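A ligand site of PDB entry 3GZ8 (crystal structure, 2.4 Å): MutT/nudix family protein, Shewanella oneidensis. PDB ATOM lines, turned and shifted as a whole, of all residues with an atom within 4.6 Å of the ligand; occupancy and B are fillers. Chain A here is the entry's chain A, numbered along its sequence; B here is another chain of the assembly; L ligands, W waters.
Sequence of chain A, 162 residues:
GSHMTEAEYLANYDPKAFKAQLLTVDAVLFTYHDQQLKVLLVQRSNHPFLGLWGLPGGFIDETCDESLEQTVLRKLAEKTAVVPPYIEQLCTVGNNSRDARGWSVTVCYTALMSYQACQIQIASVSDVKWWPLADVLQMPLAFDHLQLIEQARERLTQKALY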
ATOM      1  N   LEU A  22     -23.166 -34.020  13.729  1.00  0.00           N
ATOM      2  CA  LEU A  22     -23.336 -33.175  12.535  1.00  0.00           C
ATOM      3  C   LEU A  22     -22.352 -33.586  11.481  1.00  0.00           C
ATOM      4  O   LEU A  22     -21.188 -33.854  11.789  1.00  0.00           O
ATOM      5  CB  LEU A  22     -23.104 -31.697  12.829  1.00  0.00           C
ATOM      6  CG  LEU A  22     -23.986 -30.912  13.821  1.00  0.00           C
ATOM      7  CD1 LEU A  22     -23.910 -29.448  13.388  1.00  0.00           C
ATOM      8  CD2 LEU A  22     -25.445 -31.365  13.885  1.00  0.00           C
ATOM      9  N   THR A  24     -20.904 -32.487   7.672  1.00  0.00           N
ATOM     10  CA  THR A  24     -20.861 -31.395   6.720  1.00  0.00           C
ATOM     11  C   THR A  24     -19.726 -31.580   5.729  1.00  0.00           C
ATOM     12  O   THR A  24     -18.885 -32.479   5.898  1.00  0.00           O
ATOM     13  CB  THR A  24     -20.704 -30.023   7.423  1.00  0.00           C
ATOM     14  OG1 THR A  24     -19.556 -30.028   8.269  1.00  0.00           O
ATOM     15  CG2 THR A  24     -21.951 -29.682   8.268  1.00  0.00           C
ATOM     16  N   VAL A  25     -19.734 -30.743   4.693  1.00  0.00           N
ATOM     17  CA  VAL A  25     -18.610 -30.623   3.768  1.00  0.00           C
ATOM     18  C   VAL A  25     -18.186 -29.165   3.731  1.00  0.00           C
ATOM     19  O   VAL A  25     -18.995 -28.290   4.051  1.00  0.00           O
ATOM     20  CB  VAL A  25     -18.919 -31.129   2.347  1.00  0.00           C
ATOM     21  CG1 VAL A  25     -19.387 -32.570   2.370  1.00  0.00           C
ATOM     22  CG2 VAL A  25     -19.936 -30.245   1.656  1.00  0.00           C
ATOM     23  N   ASP A  26     -16.941 -28.906   3.351  1.00  0.00           N
ATOM     24  CA  ASP A  26     -16.456 -27.539   3.167  1.00  0.00           C
ATOM     25  C   ASP A  26     -15.539 -27.539   1.966  1.00  0.00           C
ATOM     26  O   ASP A  26     -14.991 -28.591   1.627  1.00  0.00           O
ATOM     27  CB  ASP A  26     -15.672 -27.069   4.396  1.00  0.00           C
ATOM     28  CG  ASP A  26     -16.557 -26.594   5.521  1.00  0.00           C
ATOM     29  OD1 ASP A  26     -17.301 -25.608   5.339  1.00  0.00           O
ATOM     30  OD2 ASP A  26     -16.506 -27.193   6.604  1.00  0.00           O
ATOM     31  N   ARG A  44     -22.006 -15.319   5.749  1.00  0.00           N
ATOM     32  CA  ARG A  44     -23.083 -16.141   6.346  1.00  0.00           C
ATOM     33  C   ARG A  44     -24.363 -15.347   6.699  1.00  0.00           C
ATOM     34  O   ARG A  44     -24.301 -14.284   7.320  1.00  0.00           O
ATOM     35  CB  ARG A  44     -22.554 -16.814   7.617  1.00  0.00           C
ATOM     36  CG  ARG A  44     -21.381 -17.779   7.362  1.00  0.00           C
ATOM     37  CD  ARG A  44     -20.839 -18.440   8.650  1.00  0.00           C
ATOM     38  NE  ARG A  44     -21.896 -19.043   9.440  1.00  0.00           N
ATOM     39  CZ  ARG A  44     -22.511 -20.171   9.101  1.00  0.00           C
ATOM     40  NH1 ARG A  44     -22.154 -20.842   8.000  1.00  0.00           N
ATOM     41  NH2 ARG A  44     -23.488 -20.656   9.888  1.00  0.00           N
ATOM     42  N   ASN A  46     -26.752 -17.209   8.353  1.00  0.00           N
ATOM     43  CA  ASN A  46     -27.297 -18.124   9.350  1.00  0.00           C
ATOM     44  C   ASN A  46     -26.376 -18.174  10.542  1.00  0.00           C
ATOM     45  O   ASN A  46     -25.177 -17.966  10.434  1.00  0.00           O
ATOM     46  CB  ASN A  46     -27.463 -19.541   8.764  1.00  0.00           C
ATOM     47  CG  ASN A  46     -28.625 -19.651   7.774  1.00  0.00           C
ATOM     48  OD1 ASN A  46     -29.561 -18.845   7.788  1.00  0.00           O
ATOM     49  ND2 ASN A  46     -28.571 -20.665   6.918  1.00  0.00           N
ATOM     50  N   HIS A  47     -26.953 -18.472  11.700  1.00  0.00           N
ATOM     51  CA  HIS A  47     -26.163 -18.731  12.874  1.00  0.00           C
ATOM     52  C   HIS A  47     -25.548 -20.125  12.723  1.00  0.00           C
ATOM     53  O   HIS A  47     -25.987 -20.912  11.888  1.00  0.00           O
ATOM     54  CB  HIS A  47     -27.071 -18.741  14.088  1.00  0.00           C
ATOM     55  CG  HIS A  47     -27.602 -17.396  14.463  1.00  0.00           C
ATOM     56  ND1 HIS A  47     -28.956 -17.095  14.480  1.00  0.00           N
ATOM     57  CD2 HIS A  47     -26.970 -16.265  14.882  1.00  0.00           C
ATOM     58  CE1 HIS A  47     -29.124 -15.849  14.883  1.00  0.00           C
ATOM     59  NE2 HIS A  47     -27.936 -15.322  15.118  1.00  0.00           N
ATOM     60  N   LEU A  55     -15.950 -20.382   4.765  1.00  0.00           N
ATOM     61  CA  LEU A  55     -15.921 -21.222   3.552  1.00  0.00           C
ATOM     62  C   LEU A  55     -17.313 -21.680   3.106  1.00  0.00           C
ATOM     63  O   LEU A  55     -18.173 -21.931   3.942  1.00  0.00           O
ATOM     64  CB  LEU A  55     -15.062 -22.484   3.750  1.00  0.00           C
ATOM     65  CG  LEU A  55     -13.594 -22.293   4.086  1.00  0.00           C
ATOM     66  CD1 LEU A  55     -13.013 -23.551   4.796  1.00  0.00           C
ATOM     67  CD2 LEU A  55     -12.817 -21.932   2.838  1.00  0.00           C
ATOM     68  N   GLY A  57     -19.786 -24.198   2.523  1.00  0.00           N
ATOM     69  CA  GLY A  57     -19.966 -25.585   2.946  1.00  0.00           C
ATOM     70  C   GLY A  57     -21.431 -25.932   3.159  1.00  0.00           C
ATOM     71  O   GLY A  57     -22.330 -25.240   2.626  1.00  0.00           O
ATOM     72  N   GLY A  58     -21.697 -27.006   3.916  1.00  0.00           N
ATOM     73  CA  GLY A  58     -23.077 -27.371   4.158  1.00  0.00           C
ATOM     74  C   GLY A  58     -23.372 -28.816   4.467  1.00  0.00           C
ATOM     75  O   GLY A  58     -22.467 -29.659   4.578  1.00  0.00           O
ATOM     76  N   PHE A  59     -24.676 -29.090   4.597  1.00  0.00           N
ATOM     77  CA  PHE A  59     -25.165 -30.401   4.977  1.00  0.00           C
ATOM     78  C   PHE A  59     -25.558 -31.243   3.784  1.00  0.00           C
ATOM     79  O   PHE A  59     -25.988 -30.733   2.722  1.00  0.00           O
ATOM     80  CB  PHE A  59     -26.380 -30.242   5.886  1.00  0.00           C
ATOM     81  CG  PHE A  59     -26.062 -29.621   7.202  1.00  0.00           C
ATOM     82  CD1 PHE A  59     -25.640 -30.409   8.265  1.00  0.00           C
ATOM     83  CD2 PHE A  59     -26.180 -28.233   7.377  1.00  0.00           C
ATOM     84  CE1 PHE A  59     -25.348 -29.839   9.499  1.00  0.00           C
ATOM     85  CE2 PHE A  59     -25.878 -27.644   8.591  1.00  0.00           C
ATOM     86  CZ  PHE A  59     -25.466 -28.452   9.673  1.00  0.00           C
ATOM     87  N   LYS A  75     -23.159 -27.445  -2.921  1.00  0.00           N
ATOM     88  CA  LYS A  75     -23.025 -26.329  -1.982  1.00  0.00           C
ATOM     89  C   LYS A  75     -22.279 -25.194  -2.647  1.00  0.00           C
ATOM     90  O   LYS A  75     -22.635 -24.021  -2.480  1.00  0.00           O
ATOM     91  CB  LYS A  75     -22.334 -26.743  -0.673  1.00  0.00           C
ATOM     92  CG  LYS A  75     -23.137 -27.760   0.247  1.00  0.00           C
ATOM     93  CD  LYS A  75     -24.666 -27.621   0.241  1.00  0.00           C
ATOM     94  CE  LYS A  75     -25.130 -26.248   0.797  1.00  0.00           C
ATOM     95  NZ  LYS A  75     -26.637 -26.085   0.750  1.00  0.00           N
ATOM     96  N   LYS A  79     -24.148 -21.608  -3.143  1.00  0.00           N
ATOM     97  CA  LYS A  79     -23.735 -20.414  -2.398  1.00  0.00           C
ATOM     98  C   LYS A  79     -22.834 -19.466  -3.208  1.00  0.00           C
ATOM     99  O   LYS A  79     -22.635 -18.302  -2.853  1.00  0.00           O
ATOM    100  CB  LYS A  79     -23.079 -20.794  -1.080  1.00  0.00           C
ATOM    101  CG  LYS A  79     -23.915 -21.703  -0.180  1.00  0.00           C
ATOM    102  CD  LYS A  79     -23.252 -21.878   1.168  1.00  0.00           C
ATOM    103  CE  LYS A  79     -24.205 -22.411   2.207  1.00  0.00           C
ATOM    104  NZ  LYS A  79     -23.530 -22.624   3.531  1.00  0.00           N
ATOM    105  N   ARG A  98     -15.336 -27.836  17.502  1.00  0.00           N
ATOM    106  CA  ARG A  98     -15.265 -26.953  16.330  1.00  0.00           C
ATOM    107  C   ARG A  98     -16.619 -26.274  15.992  1.00  0.00           C
ATOM    108  O   ARG A  98     -16.664 -25.198  15.371  1.00  0.00           O
ATOM    109  CB  ARG A  98     -14.675 -27.705  15.114  1.00  0.00           C
ATOM    110  CG  ARG A  98     -15.491 -28.916  14.644  1.00  0.00           C
ATOM    111  CD  ARG A  98     -15.022 -29.533  13.301  1.00  0.00           C
ATOM    112  NE  ARG A  98     -14.936 -28.493  12.276  1.00  0.00           N
ATOM    113  CZ  ARG A  98     -15.958 -28.069  11.521  1.00  0.00           C
ATOM    114  NH1 ARG A  98     -17.162 -28.640  11.616  1.00  0.00           N
ATOM    115  NH2 ARG A  98     -15.749 -27.095  10.635  1.00  0.00           N
ATOM    116  N   ASP A  99     -17.718 -26.927  16.402  1.00  0.00           N
ATOM    117  CA  ASP A  99     -19.075 -26.462  16.097  1.00  0.00           C
ATOM    118  C   ASP A  99     -19.923 -26.496  17.368  1.00  0.00           C
ATOM    119  O   ASP A  99     -20.254 -27.581  17.882  1.00  0.00           O
ATOM    120  CB  ASP A  99     -19.706 -27.345  15.010  1.00  0.00           C
ATOM    121  CG  ASP A  99     -20.887 -26.663  14.300  1.00  0.00           C
ATOM    122  OD1 ASP A  99     -21.781 -26.092  14.964  1.00  0.00           O
ATOM    123  OD2 ASP A  99     -20.924 -26.690  13.049  1.00  0.00           O
ATOM    124  N   ARG A 101     -22.969 -26.224  17.859  1.00  0.00           N
ATOM    125  CA  ARG A 101     -24.183 -27.028  17.652  1.00  0.00           C
ATOM    126  C   ARG A 101     -24.065 -28.489  18.082  1.00  0.00           C
ATOM    127  O   ARG A 101     -25.073 -29.205  18.199  1.00  0.00           O
ATOM    128  CB  ARG A 101     -24.653 -26.954  16.201  1.00  0.00           C
ATOM    129  CG  ARG A 101     -25.085 -25.575  15.779  1.00  0.00           C
ATOM    130  CD  ARG A 101     -25.442 -25.499  14.324  1.00  0.00           C
ATOM    131  NE  ARG A 101     -24.273 -25.588  13.461  1.00  0.00           N
ATOM    132  CZ  ARG A 101     -24.254 -25.199  12.186  1.00  0.00           C
ATOM    133  NH1 ARG A 101     -25.340 -24.699  11.614  1.00  0.00           N
ATOM    134  NH2 ARG A 101     -23.136 -25.337  11.482  1.00  0.00           N
ATOM    135  N   SER A 104     -19.142 -32.778  15.807  1.00  0.00           N
ATOM    136  CA  SER A 104     -19.223 -32.333  14.428  1.00  0.00           C
ATOM    137  C   SER A 104     -18.137 -32.922  13.554  1.00  0.00           C
ATOM    138  O   SER A 104     -16.981 -32.935  13.960  1.00  0.00           O
ATOM    139  CB  SER A 104     -19.094 -30.820  14.411  1.00  0.00           C
ATOM    140  OG  SER A 104     -18.635 -30.364  13.143  1.00  0.00           O
ATOM    141  N   THR A 106     -16.577 -32.480   9.598  1.00  0.00           N
ATOM    142  CA  THR A 106     -16.615 -31.857   8.276  1.00  0.00           C
ATOM    143  C   THR A 106     -15.564 -32.477   7.356  1.00  0.00           C
ATOM    144  O   THR A 106     -14.421 -32.733   7.764  1.00  0.00           O
ATOM    145  CB  THR A 106     -16.445 -30.306   8.319  1.00  0.00           C
ATOM    146  OG1 THR A 106     -16.943 -29.725   7.098  1.00  0.00           O
ATOM    147  CG2 THR A 106     -14.985 -29.905   8.493  1.00  0.00           C
ATOM    148  N   SER A 124     -29.021 -18.730   2.268  1.00  0.00           N
ATOM    149  CA  SER A 124     -28.173 -19.021   3.462  1.00  0.00           C
ATOM    150  C   SER A 124     -26.898 -18.180   3.538  1.00  0.00           C
ATOM    151  O   SER A 124     -26.207 -18.181   4.566  1.00  0.00           O
ATOM    152  CB  SER A 124     -27.830 -20.518   3.525  1.00  0.00           C
ATOM    153  OG  SER A 124     -27.250 -20.902   2.309  1.00  0.00           O
ATOM    154  N   PHE A 143     -16.273 -20.811  12.428  1.00  0.00           N
ATOM    155  CA  PHE A 143     -15.770 -22.083  12.916  1.00  0.00           C
ATOM    156  C   PHE A 143     -14.247 -22.094  12.855  1.00  0.00           C
ATOM    157  O   PHE A 143     -13.597 -21.100  13.178  1.00  0.00           O
ATOM    158  CB  PHE A 143     -16.354 -23.255  12.120  1.00  0.00           C
ATOM    159  CG  PHE A 143     -17.834 -23.144  11.878  1.00  0.00           C
ATOM    160  CD1 PHE A 143     -18.738 -23.672  12.799  1.00  0.00           C
ATOM    161  CD2 PHE A 143     -18.326 -22.492  10.741  1.00  0.00           C
ATOM    162  CE1 PHE A 143     -20.085 -23.570  12.587  1.00  0.00           C
ATOM    163  CE2 PHE A 143     -19.682 -22.379  10.516  1.00  0.00           C
ATOM    164  CZ  PHE A 143     -20.574 -22.935  11.448  1.00  0.00           C
ATOM    165  N   HIS A 145     -12.507 -22.408  10.100  1.00  0.00           N
ATOM    166  CA  HIS A 145     -12.252 -22.284   8.661  1.00  0.00           C
ATOM    167  C   HIS A 145     -10.901 -21.656   8.360  1.00  0.00           C
ATOM    168  O   HIS A 145     -10.380 -21.806   7.260  1.00  0.00           O
ATOM    169  CB  HIS A 145     -13.372 -21.521   7.944  1.00  0.00           C
ATOM    170  CG  HIS A 145     -14.666 -22.272   7.881  1.00  0.00           C
ATOM    171  ND1 HIS A 145     -15.752 -21.841   7.133  1.00  0.00           N
ATOM    172  CD2 HIS A 145     -15.053 -23.435   8.459  1.00  0.00           C
ATOM    173  CE1 HIS A 145     -16.750 -22.699   7.274  1.00  0.00           C
ATOM    174  NE2 HIS A 145     -16.347 -23.670   8.081  1.00  0.00           N
ATOM    175  N   TYR B  13     -31.345 -25.054  19.521  1.00  0.00           N
ATOM    176  CA  TYR B  13     -30.959 -25.955  18.432  1.00  0.00           C
ATOM    177  C   TYR B  13     -31.342 -27.405  18.697  1.00  0.00           C
ATOM    178  O   TYR B  13     -30.973 -27.965  19.733  1.00  0.00           O
ATOM    179  CB  TYR B  13     -29.449 -25.856  18.116  1.00  0.00           C
ATOM    180  CG  TYR B  13     -29.069 -26.698  16.932  1.00  0.00           C
ATOM    181  CD1 TYR B  13     -29.337 -26.244  15.634  1.00  0.00           C
ATOM    182  CD2 TYR B  13     -28.483 -27.979  17.087  1.00  0.00           C
ATOM    183  CE1 TYR B  13     -29.038 -27.011  14.525  1.00  0.00           C
ATOM    184  CE2 TYR B  13     -28.157 -28.760  15.978  1.00  0.00           C
ATOM    185  CZ  TYR B  13     -28.433 -28.255  14.698  1.00  0.00           C
ATOM    186  OH  TYR B  13     -28.139 -28.986  13.564  1.00  0.00           O
ATOM    187  N   PHE B  18     -33.827 -32.615  11.689  1.00  0.00           N
ATOM    188  CA  PHE B  18     -33.170 -32.929  10.416  1.00  0.00           C
ATOM    189  C   PHE B  18     -32.752 -34.373  10.321  1.00  0.00           C
ATOM    190  O   PHE B  18     -32.355 -34.972  11.319  1.00  0.00           O
ATOM    191  CB  PHE B  18     -31.958 -32.025  10.204  1.00  0.00           C
ATOM    192  CG  PHE B  18     -32.242 -30.576  10.443  1.00  0.00           C
ATOM    193  CD1 PHE B  18     -32.966 -29.837   9.513  1.00  0.00           C
ATOM    194  CD2 PHE B  18     -31.842 -29.967  11.619  1.00  0.00           C
ATOM    195  CE1 PHE B  18     -33.261 -28.488   9.737  1.00  0.00           C
ATOM    196  CE2 PHE B  18     -32.116 -28.628  11.864  1.00  0.00           C
ATOM    197  CZ  PHE B  18     -32.816 -27.885  10.934  1.00  0.00           C
ATOM    198  N   LYS B  19     -32.826 -34.937   9.114  1.00  0.00           N
ATOM    199  CA  LYS B  19     -32.320 -36.287   8.901  1.00  0.00           C
ATOM    200  C   LYS B  19     -30.799 -36.333   9.077  1.00  0.00           C
ATOM    201  O   LYS B  19     -30.092 -35.475   8.583  1.00  0.00           O
ATOM    202  CB  LYS B  19     -32.706 -36.861   7.523  1.00  0.00           C
ATOM    203  CG  LYS B  19     -32.526 -38.387   7.531  1.00  0.00           C
ATOM    204  CD  LYS B  19     -32.739 -39.041   6.200  1.00  0.00           C
ATOM    205  CE  LYS B  19     -32.621 -40.547   6.357  1.00  0.00           C
ATOM    206  NZ  LYS B  19     -31.230 -40.954   6.745  1.00  0.00           N
HETATM  207  N1  LIG L   1     -28.676 -31.413   9.311  1.00  0.00           N
HETATM  208  C1  LIG L   1     -29.219 -31.048   8.122  1.00  0.00           C
HETATM  209  N2  LIG L   1     -29.645 -29.792   7.875  1.00  0.00           N
HETATM  210  C2  LIG L   1     -29.520 -28.826   8.831  1.00  0.00           C
HETATM  211  C3  LIG L   1     -28.915 -29.165  10.129  1.00  0.00           C
HETATM  212  C4  LIG L   1     -28.500 -30.549  10.338  1.00  0.00           C
HETATM  213  N3  LIG L   1     -27.946 -30.913  11.534  1.00  0.00           N
HETATM  214  N4  LIG L   1     -28.916 -28.051  10.867  1.00  0.00           N
HETATM  215  C5  LIG L   1     -29.456 -27.060  10.115  1.00  0.00           C
HETATM  216  N5  LIG L   1     -29.835 -27.528   8.909  1.00  0.00           N
HETATM  217  C6  LIG L   1     -30.456 -26.738   7.828  1.00  0.00           C
HETATM  218  C7  LIG L   1     -31.392 -25.684   8.386  1.00  0.00           C
HETATM  219  O1  LIG L   1     -32.477 -25.492   7.456  1.00  0.00           O
HETATM  220  C8  LIG L   1     -30.567 -24.409   8.400  1.00  0.00           C
HETATM  221  O2  LIG L   1     -31.381 -23.253   8.231  1.00  0.00           O
HETATM  222  O3  LIG L   1     -29.453 -26.043   7.107  1.00  0.00           O
HETATM  223  C9  LIG L   1     -29.638 -24.638   7.225  1.00  0.00           C
HETATM  224  C10 LIG L   1     -28.253 -24.065   7.431  1.00  0.00           C
HETATM  225  O4  LIG L   1     -27.594 -24.198   6.172  1.00  0.00           O
HETATM  226  P1  LIG L   1     -26.157 -23.513   6.020  1.00  0.00           P
HETATM  227  O5  LIG L   1     -26.207 -22.064   6.476  1.00  0.00           O
HETATM  228  O6  LIG L   1     -25.670 -23.860   4.648  1.00  0.00           O
HETATM  229  O7  LIG L   1     -25.428 -24.446   7.127  1.00  0.00           O
HETATM  230  P2  LIG L   1     -24.147 -23.971   7.977  1.00  0.00           P
HETATM  231  O8  LIG L   1     -24.619 -23.282   9.204  1.00  0.00           O
HETATM  232  O9  LIG L   1     -23.253 -23.336   6.944  1.00  0.00           O
HETATM  233  O10 LIG L   1     -23.483 -25.328   8.547  1.00  0.00           O
HETATM  234  C11 LIG L   1     -22.436 -25.963   7.810  1.00  0.00           C
HETATM  235  O11 LIG L   1     -21.007 -26.129   9.742  1.00  0.00           O
HETATM  236  O12 LIG L   1     -19.525 -27.373  11.047  1.00  0.00           O
HETATM  237  C12 LIG L   1     -19.649 -26.327  10.088  1.00  0.00           C
HETATM  238  O13 LIG L   1     -17.645 -26.092   8.792  1.00  0.00           O
HETATM  239  C13 LIG L   1     -18.967 -26.663   8.779  1.00  0.00           C
HETATM  240  O14 LIG L   1     -19.287 -24.941   7.038  1.00  0.00           O
HETATM  241  C14 LIG L   1     -19.870 -26.083   7.684  1.00  0.00           C
HETATM  242  C15 LIG L   1     -21.099 -25.579   8.427  1.00  0.00           C
HETATM  243  O   HOH W   1     -27.399 -23.716   2.248  1.00  0.00           O
HETATM  244  O   HOH W   2     -24.683 -19.802   6.226  1.00  0.00           O
HETATM  245  O   HOH W   3     -26.379 -26.762   3.704  1.00  0.00           O
HETATM  246  O   HOH W   4     -28.873 -26.911   4.400  1.00  0.00           O
HETATM  247  O   HOH W   5     -29.478 -33.959  12.300  1.00  0.00           O
HETATM  248  O   HOH W   6     -20.873 -23.375   5.259  1.00  0.00           O
HETATM  249  O   HOH W   7     -27.134 -22.679  10.149  1.00  0.00           O
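Residues that only touch the ligand: Phe 59 (3.3 Å), Phe 18 of chain B (3.4 Å), Thr 24 (3.5 Å), Leu 22 (3.5 Å), Phe 143 (3.6 Å), Ser 124 (3.7 Å), Ser 104 (3.8 Å), His 47 (3.8 Å) and Gly 58 (3.97 Å). Within 4 Å of the ligand: Leu 22, Thr 24, Asp 26, Arg 44, Asn 46, His 47, Gly 58, Phe 59, Lys 79, Arg 98, Asp 99, Arg 101, Ser 104, Ser 124, Phe 143, His 145, Tyr 13 of chain B and Phe 18 of chain B. The nearest printed residue that does not touch the ligand is Thr 106 (4.04 Å).
The side-chain hydroxyl of Thr 106 is in hydrogen-bond range of the side-chain carboxylate of Asp 26. The guanidinium group of Arg 101 is in salt-bridge range of the side-chain carboxylate of Asp 99 (3.0 Å). The guanidinium group (NH2) of Arg 44 sits at hydrogen-bond distance from the backbone carbonyl oxygen (O) of His 47 (3.2 Å). The backbone carbonyl oxygen (O) of Asn 46 lies within hydrogen-bond range of the guanidinium group (NH2) of Arg 44 (3.2 Å). NH1 of Arg 98 sits at hydrogen-bond distance from OG of Ser 104. OD1 of Asp 26 sits at hydrogen-bond distance from NE2 of His 145, 3.5 Å away. The side-chain hydroxyl (OG1) of Thr 24 is in hydrogen-bond range of the side-chain hydroxyl (OG1) of Thr 106. The backbone carbonyl oxygen (O) of Gly 57 lies within hydrogen-bond range of the side-chain amino group (NZ) of Lys 79, 3.0 Å away.
Water W2 lies within hydrogen-bond range of O5 of the ligand (2.7 Å), O of Ser 124 (2.8 Å) and NH1 of Arg 44 (3.3 Å). Water W7 lies within hydrogen-bond range of O of His 47, O8 of the ligand and NH1 of Arg 101. Water W6 lies within hydrogen-bond range of O14 of the ligand (2.9 Å), N of Gly 57 (3.1 Å), NZ of Lys 79 (3.3 Å) and O of Leu 55 (3.3 Å). Water W1 lies within hydrogen-bond range of the side-chain hydroxyl (OG) of Ser 124 (2.8 Å), the side-chain amino group (NZ) of Lys 75 (2.9 Å) and an oxygen (O6) of the ligand (3.0 Å). Water W3 lies within hydrogen-bond range of the backbone NH of Phe 59 (3.0 Å), the side-chain amino group of Lys 75 (3.0 Å) and an oxygen (O6) of the ligand (3.1 Å). Water W5 lies within hydrogen-bond range of the backbone carbonyl oxygen of Phe 18 of chain B (3.2 Å) and a nitrogen (N3) of the ligand (3.5 Å).
The guanidinium group (NH1) of Arg 98 sits at hydrogen-bond distance from an oxygen (O12) of the ligand, 2.7 Å away. OH of Tyr 13 of chain B lies within hydrogen-bond range of N3 of the ligand, at 2.8 Å. The side-chain amino group (NZ) of Lys 79 is in salt-bridge range of an oxygen (O6) of the ligand (2.7 Å). An oxygen (O5) of the ligand lies within hydrogen-bond range of the side-chain amide nitrogen (ND2) of Asn 46 (2.8 Å). An oxygen (O8) of the ligand is in salt-bridge range of the guanidinium group of Arg 101, 2.9 Å away. O9 of the ligand is in salt-bridge range of NH1 of Arg 44, at 2.9 Å. The side-chain carboxylate (OD1) of Asp 26 lies within hydrogen-bond range of an oxygen (O14) of the ligand (2.7 Å). An oxygen (O12) of the ligand lies within hydrogen-bond range of the side-chain carboxylate (OD2) of Asp 99 (2.5 Å). An oxygen (O13) of the ligand sits at hydrogen-bond distance from a ring nitrogen (NE2) of His 145, 2.8 Å away.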
